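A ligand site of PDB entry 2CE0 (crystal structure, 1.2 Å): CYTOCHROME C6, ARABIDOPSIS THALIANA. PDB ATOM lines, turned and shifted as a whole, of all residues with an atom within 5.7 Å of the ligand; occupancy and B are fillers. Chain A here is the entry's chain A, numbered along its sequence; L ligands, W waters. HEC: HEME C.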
ATOM      1  N   PHE A  12      -5.922 -25.283  22.559  1.00  0.00           N
ATOM      2  CA  PHE A  12      -4.682 -25.511  21.816  1.00  0.00           C
ATOM      3  C   PHE A  12      -3.957 -26.734  22.344  1.00  0.00           C
ATOM      4  O   PHE A  12      -3.468 -27.560  21.547  1.00  0.00           O
ATOM      5  CB  PHE A  12      -3.768 -24.286  21.898  1.00  0.00           C
ATOM      6  CG  PHE A  12      -2.484 -24.453  21.121  1.00  0.00           C
ATOM      7  CD1 PHE A  12      -2.399 -24.070  19.783  1.00  0.00           C
ATOM      8  CD2 PHE A  12      -1.348 -25.009  21.724  1.00  0.00           C
ATOM      9  CE1 PHE A  12      -1.214 -24.254  19.054  1.00  0.00           C
ATOM     10  CE2 PHE A  12      -0.161 -25.182  21.002  1.00  0.00           C
ATOM     11  CZ  PHE A  12      -0.105 -24.801  19.668  1.00  0.00           C
ATOM     12  N   ALA A  15      -6.011 -29.860  21.093  1.00  0.00           N
ATOM     13  CA  ALA A  15      -6.268 -30.034  19.657  1.00  0.00           C
ATOM     14  C   ALA A  15      -5.057 -29.854  18.754  1.00  0.00           C
ATOM     15  O   ALA A  15      -5.093 -30.256  17.591  1.00  0.00           O
ATOM     16  CB  ALA A  15      -7.410 -29.117  19.203  1.00  0.00           C
ATOM     17  N   CYS A  16      -4.005 -29.229  19.281  1.00  0.00           N
ATOM     18  CA  CYS A  16      -2.886 -28.768  18.437  1.00  0.00           C
ATOM     19  C   CYS A  16      -1.494 -29.117  18.951  1.00  0.00           C
ATOM     20  O   CYS A  16      -0.576 -29.304  18.155  1.00  0.00           O
ATOM     21  CB  CYS A  16      -2.936 -27.247  18.220  1.00  0.00           C
ATOM     22  SG  CYS A  16      -4.575 -26.558  17.869  1.00  0.00           S
ATOM     23  N   CYS A  19       1.276 -31.844  17.802  1.00  0.00           N
ATOM     24  CA  CYS A  19       2.032 -31.546  16.588  1.00  0.00           C
ATOM     25  C   CYS A  19       2.814 -30.259  16.679  1.00  0.00           C
ATOM     26  O   CYS A  19       3.925 -30.162  16.155  1.00  0.00           O
ATOM     27  CB  CYS A  19       1.137 -31.519  15.376  1.00  0.00           C
ATOM     28  SG  CYS A  19       0.426 -33.136  15.020  1.00  0.00           S
ATOM     29  N   HIS A  20       2.250 -29.260  17.360  1.00  0.00           N
ATOM     30  CA  HIS A  20       2.847 -27.931  17.411  1.00  0.00           C
ATOM     31  C   HIS A  20       3.372 -27.673  18.806  1.00  0.00           C
ATOM     32  O   HIS A  20       3.029 -26.673  19.433  1.00  0.00           O
ATOM     33  CB  HIS A  20       1.845 -26.862  16.980  1.00  0.00           C
ATOM     34  CG  HIS A  20       1.462 -26.957  15.537  1.00  0.00           C
ATOM     35  ND1 HIS A  20       2.370 -26.711  14.523  1.00  0.00           N
ATOM     36  CD2 HIS A  20       0.284 -27.236  14.939  1.00  0.00           C
ATOM     37  CE1 HIS A  20       1.748 -26.840  13.362  1.00  0.00           C
ATOM     38  NE2 HIS A  20       0.476 -27.139  13.581  1.00  0.00           N
ATOM     39  N   ASN A  25       6.796 -27.643  15.295  1.00  0.00           N
ATOM     40  CA  ASN A  25       6.146 -28.544  14.348  1.00  0.00           C
ATOM     41  C   ASN A  25       6.929 -29.846  14.339  1.00  0.00           C
ATOM     42  O   ASN A  25       8.026 -29.906  13.794  1.00  0.00           O
ATOM     43  CB  ASN A  25       6.048 -27.964  12.934  1.00  0.00           C
ATOM     44  CG  ASN A  25       5.116 -28.756  12.051  1.00  0.00           C
ATOM     45  OD1 ASN A  25       5.091 -29.983  12.129  1.00  0.00           O
ATOM     46  ND2 ASN A  25       4.341 -28.065  11.237  1.00  0.00           N
ATOM     47  N   ILE A  27       6.389 -32.591  12.856  1.00  0.00           N
ATOM     48  CA  ILE A  27       6.219 -33.315  11.591  1.00  0.00           C
ATOM     49  C   ILE A  27       7.020 -32.671  10.457  1.00  0.00           C
ATOM     50  O   ILE A  27       7.682 -33.359   9.674  1.00  0.00           O
ATOM     51  CB  ILE A  27       4.707 -33.350  11.180  1.00  0.00           C
ATOM     52  CG1 ILE A  27       3.844 -34.033  12.258  1.00  0.00           C
ATOM     53  CG2 ILE A  27       4.500 -33.959   9.775  1.00  0.00           C
ATOM     54  CD1 ILE A  27       4.318 -35.442  12.682  1.00  0.00           C
ATOM     55  N   GLN A  28       6.926 -31.341  10.389  1.00  0.00           N
ATOM     56  CA  GLN A  28       7.444 -30.602   9.246  1.00  0.00           C
ATOM     57  C   GLN A  28       8.330 -29.430   9.680  1.00  0.00           C
ATOM     58  O   GLN A  28       7.814 -28.372  10.056  1.00  0.00           O
ATOM     59  CB  GLN A  28       6.303 -30.104   8.368  1.00  0.00           C
ATOM     60  CG  GLN A  28       6.768 -29.441   7.076  1.00  0.00           C
ATOM     61  CD  GLN A  28       5.663 -29.311   6.059  1.00  0.00           C
ATOM     62  OE1 GLN A  28       4.766 -30.143   5.989  1.00  0.00           O
ATOM     63  NE2 GLN A  28       5.726 -28.259   5.256  1.00  0.00           N
ATOM     64  N   GLY A  30      10.424 -26.105   9.442  1.00  0.00           N
ATOM     65  CA  GLY A  30      10.187 -24.901   8.661  1.00  0.00           C
ATOM     66  C   GLY A  30       8.749 -24.428   8.638  1.00  0.00           C
ATOM     67  O   GLY A  30       8.458 -23.367   8.093  1.00  0.00           O
ATOM     68  N   ALA A  31       7.843 -25.206   9.236  1.00  0.00           N
ATOM     69  CA  ALA A  31       6.422 -24.840   9.246  1.00  0.00           C
ATOM     70  C   ALA A  31       5.892 -24.750  10.669  1.00  0.00           C
ATOM     71  O   ALA A  31       4.808 -25.258  10.990  1.00  0.00           O
ATOM     72  CB  ALA A  31       5.608 -25.804   8.391  1.00  0.00           C
ATOM     73  N   THR A  32       6.662 -24.095  11.518  1.00  0.00           N
ATOM     74  CA  THR A  32       6.265 -23.909  12.906  1.00  0.00           C
ATOM     75  C   THR A  32       5.287 -22.738  13.057  1.00  0.00           C
ATOM     76  O   THR A  32       4.950 -22.048  12.090  1.00  0.00           O
ATOM     77  CB  THR A  32       7.478 -23.644  13.836  1.00  0.00           C
ATOM     78  OG1 THR A  32       7.978 -22.321  13.602  1.00  0.00           O
ATOM     79  CG2 THR A  32       8.582 -24.689  13.648  1.00  0.00           C
ATOM     80  N   LEU A  33       4.870 -22.503  14.290  1.00  0.00           N
ATOM     81  CA  LEU A  33       3.993 -21.388  14.608  1.00  0.00           C
ATOM     82  C   LEU A  33       4.765 -20.172  15.095  1.00  0.00           C
ATOM     83  O   LEU A  33       4.159 -19.233  15.624  1.00  0.00           O
ATOM     84  CB  LEU A  33       2.917 -21.802  15.609  1.00  0.00           C
ATOM     85  CG  LEU A  33       2.179 -23.102  15.281  1.00  0.00           C
ATOM     86  CD1 LEU A  33       1.105 -23.347  16.319  1.00  0.00           C
ATOM     87  CD2 LEU A  33       1.579 -23.131  13.869  1.00  0.00           C
ATOM     88  N   PHE A  34       6.080 -20.176  14.913  1.00  0.00           N
ATOM     89  CA  PHE A  34       6.890 -18.995  15.226  1.00  0.00           C
ATOM     90  C   PHE A  34       6.730 -17.958  14.120  1.00  0.00           C
ATOM     91  O   PHE A  34       6.538 -18.298  12.937  1.00  0.00           O
ATOM     92  CB  PHE A  34       8.370 -19.360  15.384  1.00  0.00           C
ATOM     93  CG  PHE A  34       8.707 -20.023  16.702  1.00  0.00           C
ATOM     94  CD1 PHE A  34       9.242 -19.284  17.746  1.00  0.00           C
ATOM     95  CD2 PHE A  34       8.469 -21.373  16.892  1.00  0.00           C
ATOM     96  CE1 PHE A  34       9.541 -19.897  18.970  1.00  0.00           C
ATOM     97  CE2 PHE A  34       8.770 -21.990  18.107  1.00  0.00           C
ATOM     98  CZ  PHE A  34       9.311 -21.243  19.150  1.00  0.00           C
ATOM     99  N   ASP A  37       8.579 -18.371  10.596  1.00  0.00           N
ATOM    100  CA  ASP A  37       8.022 -19.390   9.727  1.00  0.00           C
ATOM    101  C   ASP A  37       6.653 -18.999   9.193  1.00  0.00           C
ATOM    102  O   ASP A  37       6.362 -19.189   8.017  1.00  0.00           O
ATOM    103  CB  ASP A  37       7.926 -20.735  10.444  1.00  0.00           C
ATOM    104  CG  ASP A  37       9.276 -21.439  10.575  1.00  0.00           C
ATOM    105  OD1 ASP A  37      10.296 -20.963  10.030  1.00  0.00           O
ATOM    106  OD2 ASP A  37       9.280 -22.506  11.225  1.00  0.00           O
ATOM    107  N   LEU A  38       5.794 -18.453  10.056  1.00  0.00           N
ATOM    108  CA  LEU A  38       4.490 -17.981   9.606  1.00  0.00           C
ATOM    109  C   LEU A  38       4.661 -16.958   8.468  1.00  0.00           C
ATOM    110  O   LEU A  38       3.965 -17.021   7.440  1.00  0.00           O
ATOM    111  CB  LEU A  38       3.697 -17.394  10.756  1.00  0.00           C
ATOM    112  CG  LEU A  38       3.246 -18.353  11.865  1.00  0.00           C
ATOM    113  CD1 LEU A  38       2.714 -17.564  13.038  1.00  0.00           C
ATOM    114  CD2 LEU A  38       2.204 -19.368  11.377  1.00  0.00           C
ATOM    115  N   ASN A  41       5.848 -18.446   5.123  1.00  0.00           N
ATOM    116  CA  ASN A  41       4.765 -19.233   4.550  1.00  0.00           C
ATOM    117  C   ASN A  41       3.538 -18.400   4.184  1.00  0.00           C
ATOM    118  O   ASN A  41       2.532 -18.930   3.743  1.00  0.00           O
ATOM    119  CB  ASN A  41       4.355 -20.347   5.530  1.00  0.00           C
ATOM    120  CG  ASN A  41       5.333 -21.513   5.542  1.00  0.00           C
ATOM    121  OD1 ASN A  41       6.199 -21.617   6.423  1.00  0.00           O
ATOM    122  ND2 ASN A  41       5.192 -22.417   4.582  1.00  0.00           N
ATOM    123  N   VAL A  43       1.479 -16.619   6.149  1.00  0.00           N
ATOM    124  CA  VAL A  43       0.325 -16.862   7.012  1.00  0.00           C
ATOM    125  C   VAL A  43       0.420 -16.245   8.417  1.00  0.00           C
ATOM    126  O   VAL A  43      -0.205 -16.726   9.360  1.00  0.00           O
ATOM    127  CB  VAL A  43      -0.028 -18.383   7.105  1.00  0.00           C
ATOM    128  CG1 VAL A  43      -0.473 -18.909   5.741  1.00  0.00           C
ATOM    129  CG2 VAL A  43       1.147 -19.193   7.658  1.00  0.00           C
ATOM    130  N   ILE A  49      -4.139 -17.767   9.644  1.00  0.00           N
ATOM    131  CA  ILE A  49      -4.049 -18.851  10.618  1.00  0.00           C
ATOM    132  C   ILE A  49      -5.409 -19.562  10.704  1.00  0.00           C
ATOM    133  O   ILE A  49      -5.481 -20.792  10.716  1.00  0.00           O
ATOM    134  CB  ILE A  49      -3.582 -18.350  12.007  1.00  0.00           C
ATOM    135  CG1 ILE A  49      -2.120 -17.890  11.930  1.00  0.00           C
ATOM    136  CG2 ILE A  49      -3.760 -19.447  13.061  1.00  0.00           C
ATOM    137  CD1 ILE A  49      -1.708 -16.933  13.038  1.00  0.00           C
ATOM    138  N   VAL A  52      -5.896 -21.773   7.413  1.00  0.00           N
ATOM    139  CA  VAL A  52      -5.169 -23.036   7.387  1.00  0.00           C
ATOM    140  C   VAL A  52      -5.701 -24.021   8.442  1.00  0.00           C
ATOM    141  O   VAL A  52      -5.753 -25.227   8.186  1.00  0.00           O
ATOM    142  CB  VAL A  52      -3.633 -22.839   7.415  1.00  0.00           C
ATOM    143  CG1 VAL A  52      -3.172 -22.304   8.758  1.00  0.00           C
ATOM    144  CG2 VAL A  52      -2.908 -24.136   7.061  1.00  0.00           C
ATOM    145  N   THR A  53      -6.130 -23.527   9.596  1.00  0.00           N
ATOM    146  CA  THR A  53      -6.717 -24.389  10.613  1.00  0.00           C
ATOM    147  C   THR A  53      -8.040 -24.972  10.113  1.00  0.00           C
ATOM    148  O   THR A  53      -8.350 -26.142  10.372  1.00  0.00           O
ATOM    149  CB  THR A  53      -6.911 -23.623  11.935  1.00  0.00           C
ATOM    150  OG1 THR A  53      -5.650 -23.098  12.353  1.00  0.00           O
ATOM    151  CG2 THR A  53      -7.424 -24.551  13.028  1.00  0.00           C
ATOM    152  N   LYS A  57      -3.637 -28.091   5.224  1.00  0.00           N
ATOM    153  CA  LYS A  57      -2.625 -27.927   4.179  1.00  0.00           C
ATOM    154  C   LYS A  57      -1.640 -29.062   4.323  1.00  0.00           C
ATOM    155  O   LYS A  57      -1.061 -29.245   5.393  1.00  0.00           O
ATOM    156  CB  LYS A  57      -1.909 -26.588   4.289  1.00  0.00           C
ATOM    157  CG  LYS A  57      -0.796 -26.424   3.248  1.00  0.00           C
ATOM    158  CD  LYS A  57      -0.107 -25.072   3.379  1.00  0.00           C
ATOM    159  CE  LYS A  57       1.064 -24.937   2.418  1.00  0.00           C
ATOM    160  NZ  LYS A  57       0.626 -25.035   1.006  1.00  0.00           N
ATOM    161  N   GLY A  58      -1.450 -29.806   3.245  1.00  0.00           N
ATOM    162  CA  GLY A  58      -0.578 -30.952   3.211  1.00  0.00           C
ATOM    163  C   GLY A  58      -0.878 -31.935   4.323  1.00  0.00           C
ATOM    164  O   GLY A  58      -2.013 -32.400   4.463  1.00  0.00           O
ATOM    165  N   ARG A  59       0.134 -32.195   5.147  1.00  0.00           N
ATOM    166  CA  ARG A  59       0.007 -33.180   6.194  1.00  0.00           C
ATOM    167  C   ARG A  59      -0.788 -32.683   7.387  1.00  0.00           C
ATOM    168  O   ARG A  59      -1.134 -33.472   8.273  1.00  0.00           O
ATOM    169  CB  ARG A  59       1.385 -33.682   6.640  1.00  0.00           C
ATOM    170  CG  ARG A  59       1.941 -34.737   5.692  1.00  0.00           C
ATOM    171  CD  ARG A  59       3.279 -35.279   6.166  1.00  0.00           C
ATOM    172  NE  ARG A  59       4.360 -34.321   5.950  1.00  0.00           N
ATOM    173  CZ  ARG A  59       5.641 -34.559   6.208  1.00  0.00           C
ATOM    174  NH1 ARG A  59       6.028 -35.740   6.690  1.00  0.00           N
ATOM    175  NH2 ARG A  59       6.549 -33.613   5.986  1.00  0.00           N
ATOM    176  N   MET A  60      -1.117 -31.390   7.404  1.00  0.00           N
ATOM    177  CA  MET A  60      -2.003 -30.920   8.431  1.00  0.00           C
ATOM    178  C   MET A  60      -3.464 -31.038   8.041  1.00  0.00           C
ATOM    179  O   MET A  60      -3.911 -30.408   7.059  1.00  0.00           O
ATOM    180  CB  MET A  60      -1.777 -29.488   8.767  1.00  0.00           C
ATOM    181  CG  MET A  60      -2.861 -29.108   9.734  1.00  0.00           C
ATOM    182  SD  MET A  60      -2.513 -27.604  10.545  1.00  0.00           S
ATOM    183  CE  MET A  60      -4.116 -26.957  11.007  1.00  0.00           C
ATOM    184  N   PRO A  61      -4.233 -31.767   8.843  1.00  0.00           N
ATOM    185  CA  PRO A  61      -5.664 -31.832   8.594  1.00  0.00           C
ATOM    186  C   PRO A  61      -6.366 -30.504   8.865  1.00  0.00           C
ATOM    187  O   PRO A  61      -5.957 -29.717   9.728  1.00  0.00           O
ATOM    188  CB  PRO A  61      -6.146 -32.892   9.579  1.00  0.00           C
ATOM    189  CG  PRO A  61      -5.138 -32.862  10.666  1.00  0.00           C
ATOM    190  CD  PRO A  61      -3.847 -32.580  10.021  1.00  0.00           C
ATOM    191  N   PHE A  63     -10.013 -28.561  10.151  1.00  0.00           N
ATOM    192  CA  PHE A  63     -10.681 -28.801  11.420  1.00  0.00           C
ATOM    193  C   PHE A  63     -12.081 -28.181  11.253  1.00  0.00           C
ATOM    194  O   PHE A  63     -12.973 -28.385  12.081  1.00  0.00           O
ATOM    195  CB  PHE A  63      -9.979 -28.239  12.649  1.00  0.00           C
ATOM    196  CG  PHE A  63      -8.854 -29.091  13.118  1.00  0.00           C
ATOM    197  CD1 PHE A  63      -9.064 -30.127  14.031  1.00  0.00           C
ATOM    198  CD2 PHE A  63      -7.587 -28.879  12.613  1.00  0.00           C
ATOM    199  CE1 PHE A  63      -7.994 -30.920  14.453  1.00  0.00           C
ATOM    200  CE2 PHE A  63      -6.530 -29.666  13.018  1.00  0.00           C
ATOM    201  CZ  PHE A  63      -6.723 -30.687  13.942  1.00  0.00           C
ATOM    202  N   LEU A  79     -14.070 -28.732  14.652  1.00  0.00           N
ATOM    203  CA  LEU A  79     -14.175 -27.614  15.580  1.00  0.00           C
ATOM    204  C   LEU A  79     -15.183 -26.609  15.051  1.00  0.00           C
ATOM    205  O   LEU A  79     -15.327 -26.423  13.838  1.00  0.00           O
ATOM    206  CB  LEU A  79     -12.808 -26.946  15.763  1.00  0.00           C
ATOM    207  CG  LEU A  79     -11.735 -27.761  16.490  1.00  0.00           C
ATOM    208  CD1 LEU A  79     -10.367 -27.139  16.297  1.00  0.00           C
ATOM    209  CD2 LEU A  79     -12.040 -27.916  17.973  1.00  0.00           C
ATOM    210  N   LEU A  87      -8.607 -20.199  18.599  1.00  0.00           N
ATOM    211  CA  LEU A  87      -7.291 -20.777  18.312  1.00  0.00           C
ATOM    212  C   LEU A  87      -6.427 -19.865  17.456  1.00  0.00           C
ATOM    213  O   LEU A  87      -5.232 -19.698  17.717  1.00  0.00           O
ATOM    214  CB  LEU A  87      -7.439 -22.157  17.681  1.00  0.00           C
ATOM    215  CG  LEU A  87      -7.874 -23.238  18.675  1.00  0.00           C
ATOM    216  CD1 LEU A  87      -8.380 -24.461  17.928  1.00  0.00           C
ATOM    217  CD2 LEU A  87      -6.732 -23.585  19.618  1.00  0.00           C
ATOM    218  N   ALA A  88      -7.015 -19.280  16.411  1.00  0.00           N
ATOM    219  CA  ALA A  88      -6.256 -18.379  15.543  1.00  0.00           C
ATOM    220  C   ALA A  88      -5.754 -17.150  16.308  1.00  0.00           C
ATOM    221  O   ALA A  88      -4.604 -16.727  16.134  1.00  0.00           O
ATOM    222  CB  ALA A  88      -7.100 -17.974  14.336  1.00  0.00           C
ATOM    223  N   VAL A  91      -2.893 -18.365  18.666  1.00  0.00           N
ATOM    224  CA  VAL A  91      -1.655 -18.627  17.935  1.00  0.00           C
ATOM    225  C   VAL A  91      -0.964 -17.310  17.543  1.00  0.00           C
ATOM    226  O   VAL A  91       0.245 -17.159  17.703  1.00  0.00           O
ATOM    227  CB  VAL A  91      -1.896 -19.530  16.708  1.00  0.00           C
ATOM    228  CG1 VAL A  91      -0.685 -19.564  15.809  1.00  0.00           C
ATOM    229  CG2 VAL A  91      -2.266 -20.939  17.139  1.00  0.00           C
HETATM  230 FE   HEC L   1      -0.939 -27.405  12.172  1.00  0.00          FE
HETATM  231  CHA HEC L   1       0.900 -25.975   9.713  1.00  0.00           C
HETATM  232  CHB HEC L   1      -2.117 -24.328  13.098  1.00  0.00           C
HETATM  233  CHC HEC L   1      -3.113 -28.889  14.347  1.00  0.00           C
HETATM  234  CHD HEC L   1       0.547 -30.418  11.595  1.00  0.00           C
HETATM  235  NA  HEC L   1      -0.677 -25.514  11.523  1.00  0.00           N
HETATM  236  C1A HEC L   1       0.172 -25.123  10.507  1.00  0.00           C
HETATM  237  C2A HEC L   1       0.163 -23.686  10.408  1.00  0.00           C
HETATM  238  C3A HEC L   1      -0.688 -23.234  11.341  1.00  0.00           C
HETATM  239  C4A HEC L   1      -1.230 -24.374  12.056  1.00  0.00           C
HETATM  240  CMA HEC L   1      -1.061 -21.765  11.654  1.00  0.00           C
HETATM  241  CAA HEC L   1       1.038 -22.884   9.409  1.00  0.00           C
HETATM  242  CBA HEC L   1       2.470 -22.819   9.998  1.00  0.00           C
HETATM  243  CGA HEC L   1       3.525 -22.281   9.045  1.00  0.00           C
HETATM  244  O1A HEC L   1       3.258 -22.205   7.831  1.00  0.00           O
HETATM  245  O2A HEC L   1       4.665 -21.948   9.504  1.00  0.00           O
HETATM  246  NB  HEC L   1      -2.328 -26.732  13.490  1.00  0.00           N
HETATM  247  C1B HEC L   1      -2.659 -25.417  13.751  1.00  0.00           C
HETATM  248  C2B HEC L   1      -3.679 -25.389  14.777  1.00  0.00           C
HETATM  249  C3B HEC L   1      -3.955 -26.663  15.093  1.00  0.00           C
HETATM  250  C4B HEC L   1      -3.117 -27.519  14.307  1.00  0.00           C
HETATM  251  CMB HEC L   1      -4.287 -24.079  15.331  1.00  0.00           C
HETATM  252  CAB HEC L   1      -5.001 -27.158  16.110  1.00  0.00           C
HETATM  253  CBB HEC L   1      -6.317 -26.888  15.887  1.00  0.00           C
HETATM  254  NC  HEC L   1      -1.225 -29.299  12.837  1.00  0.00           N
HETATM  255  C1C HEC L   1      -2.189 -29.702  13.731  1.00  0.00           C
HETATM  256  C2C HEC L   1      -2.017 -31.105  13.989  1.00  0.00           C
HETATM  257  C3C HEC L   1      -0.992 -31.527  13.242  1.00  0.00           C
HETATM  258  C4C HEC L   1      -0.480 -30.394  12.500  1.00  0.00           C
HETATM  259  CMC HEC L   1      -2.886 -31.927  14.975  1.00  0.00           C
HETATM  260  CAC HEC L   1      -0.395 -32.941  13.174  1.00  0.00           C
HETATM  261  CBC HEC L   1      -1.152 -34.028  12.905  1.00  0.00           C
HETATM  262  ND  HEC L   1       0.475 -28.077  10.882  1.00  0.00           N
HETATM  263  C1D HEC L   1       0.905 -29.389  10.765  1.00  0.00           C
HETATM  264  C2D HEC L   1       1.770 -29.535   9.634  1.00  0.00           C
HETATM  265  C3D HEC L   1       1.865 -28.162   9.060  1.00  0.00           C
HETATM  266  C4D HEC L   1       1.053 -27.319   9.879  1.00  0.00           C
HETATM  267  CMD HEC L   1       2.441 -30.806   9.136  1.00  0.00           C
HETATM  268  CAD HEC L   1       2.666 -27.778   7.814  1.00  0.00           C
HETATM  269  CBD HEC L   1       1.734 -27.851   6.598  1.00  0.00           C
HETATM  270  CGD HEC L   1       2.465 -27.442   5.347  1.00  0.00           C
HETATM  271  O1D HEC L   1       2.753 -28.337   4.525  1.00  0.00           O
HETATM  272  O2D HEC L   1       2.730 -26.217   5.199  1.00  0.00           O
HETATM  273  O   HOH W   1       2.688 -31.047   4.870  1.00  0.00           O
HETATM  274  O   HOH W   2       5.210 -25.100   4.115  1.00  0.00           O
HETATM  275  O   HOH W   3       1.705 -23.956   6.150  1.00  0.00           O
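The side-chain sulfur of Cys 16 is bonded to a carbon (CAB) of the ligand, at 1.9 Å.
An iron atom (FE) of the ligand is bound by a ring nitrogen (NE2) of His 20.
SG of Cys 19 is bonded to CAC of the ligand.
An iron atom (FE) of the ligand is bound by the side-chain sulfur of Met 60 (2.3 Å).
The backbone carbonyl oxygen (O) of Thr 32 sits close to an oxygen (O2A) of the ligand, 2.6 Å away.
An oxygen (O1D) of the ligand lies within hydrogen-bond range of the side-chain amide nitrogen (NE2) of Gln 28 (3.1 Å).
OD1 of Asn 41 sits close to O1A of the ligand.
The side-chain carboxylate (OD2) of Asp 37 sits at hydrogen-bond distance from the side-chain hydroxyl (OG1) of Thr 32 (2.7 Å).
The side-chain amide oxygen (OD1) of Asn 41 sits close to the backbone carbonyl oxygen (O) of Asp 37, at 2.9 Å.
O of Ala 31 lies within hydrogen-bond range of ND2 of Asn 25, at 2.9 Å.
The side-chain amide oxygen of Asn 25 lies within hydrogen-bond range of the backbone NH of Ile 27, 3.0 Å away.
The backbone carbonyl oxygen of Thr 53 lies within hydrogen-bond range of the backbone NH of Phe 63.
O of Ile 49 sits at hydrogen-bond distance from OG1 of Thr 53 (2.8 Å).
The backbone carbonyl oxygen (O) of Leu 38 sits at hydrogen-bond distance from the backbone NH (N) of Val 43 (2.8 Å).
O of Phe 63 lies within hydrogen-bond range of N of Leu 79.
Merely in contact with the ligand: Ala 15 (3.4 Å), Asn 25 (3.3 Å), Ile 27 (3.8 Å), Ala 31 (3.3 Å), Leu 33 (3.4 Å), Asp 37 (3.6 Å), Leu 38 (3.7 Å), Val 43 (3.7 Å), Ile 49 (3.8 Å), Val 52 (3.6 Å), Thr 53 (3.4 Å), Lys 57 (3.3 Å), Arg 59 (3.95 Å), Phe 63 (3.7 Å) and Leu 87 (3.8 Å).
Of the 30 residues printed, 22 come within 4 Å of the ligand.
The nearest printed residue that does not touch the ligand is Leu 79 (4.1 Å).
Water W1 lies within hydrogen-bond range of OE1 of Gln 28, O1D of the ligand and N of Arg 59.
Water W2 lies within hydrogen-bond range of ND2 of Asn 41, O2D of the ligand and NE2 of Gln 28.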
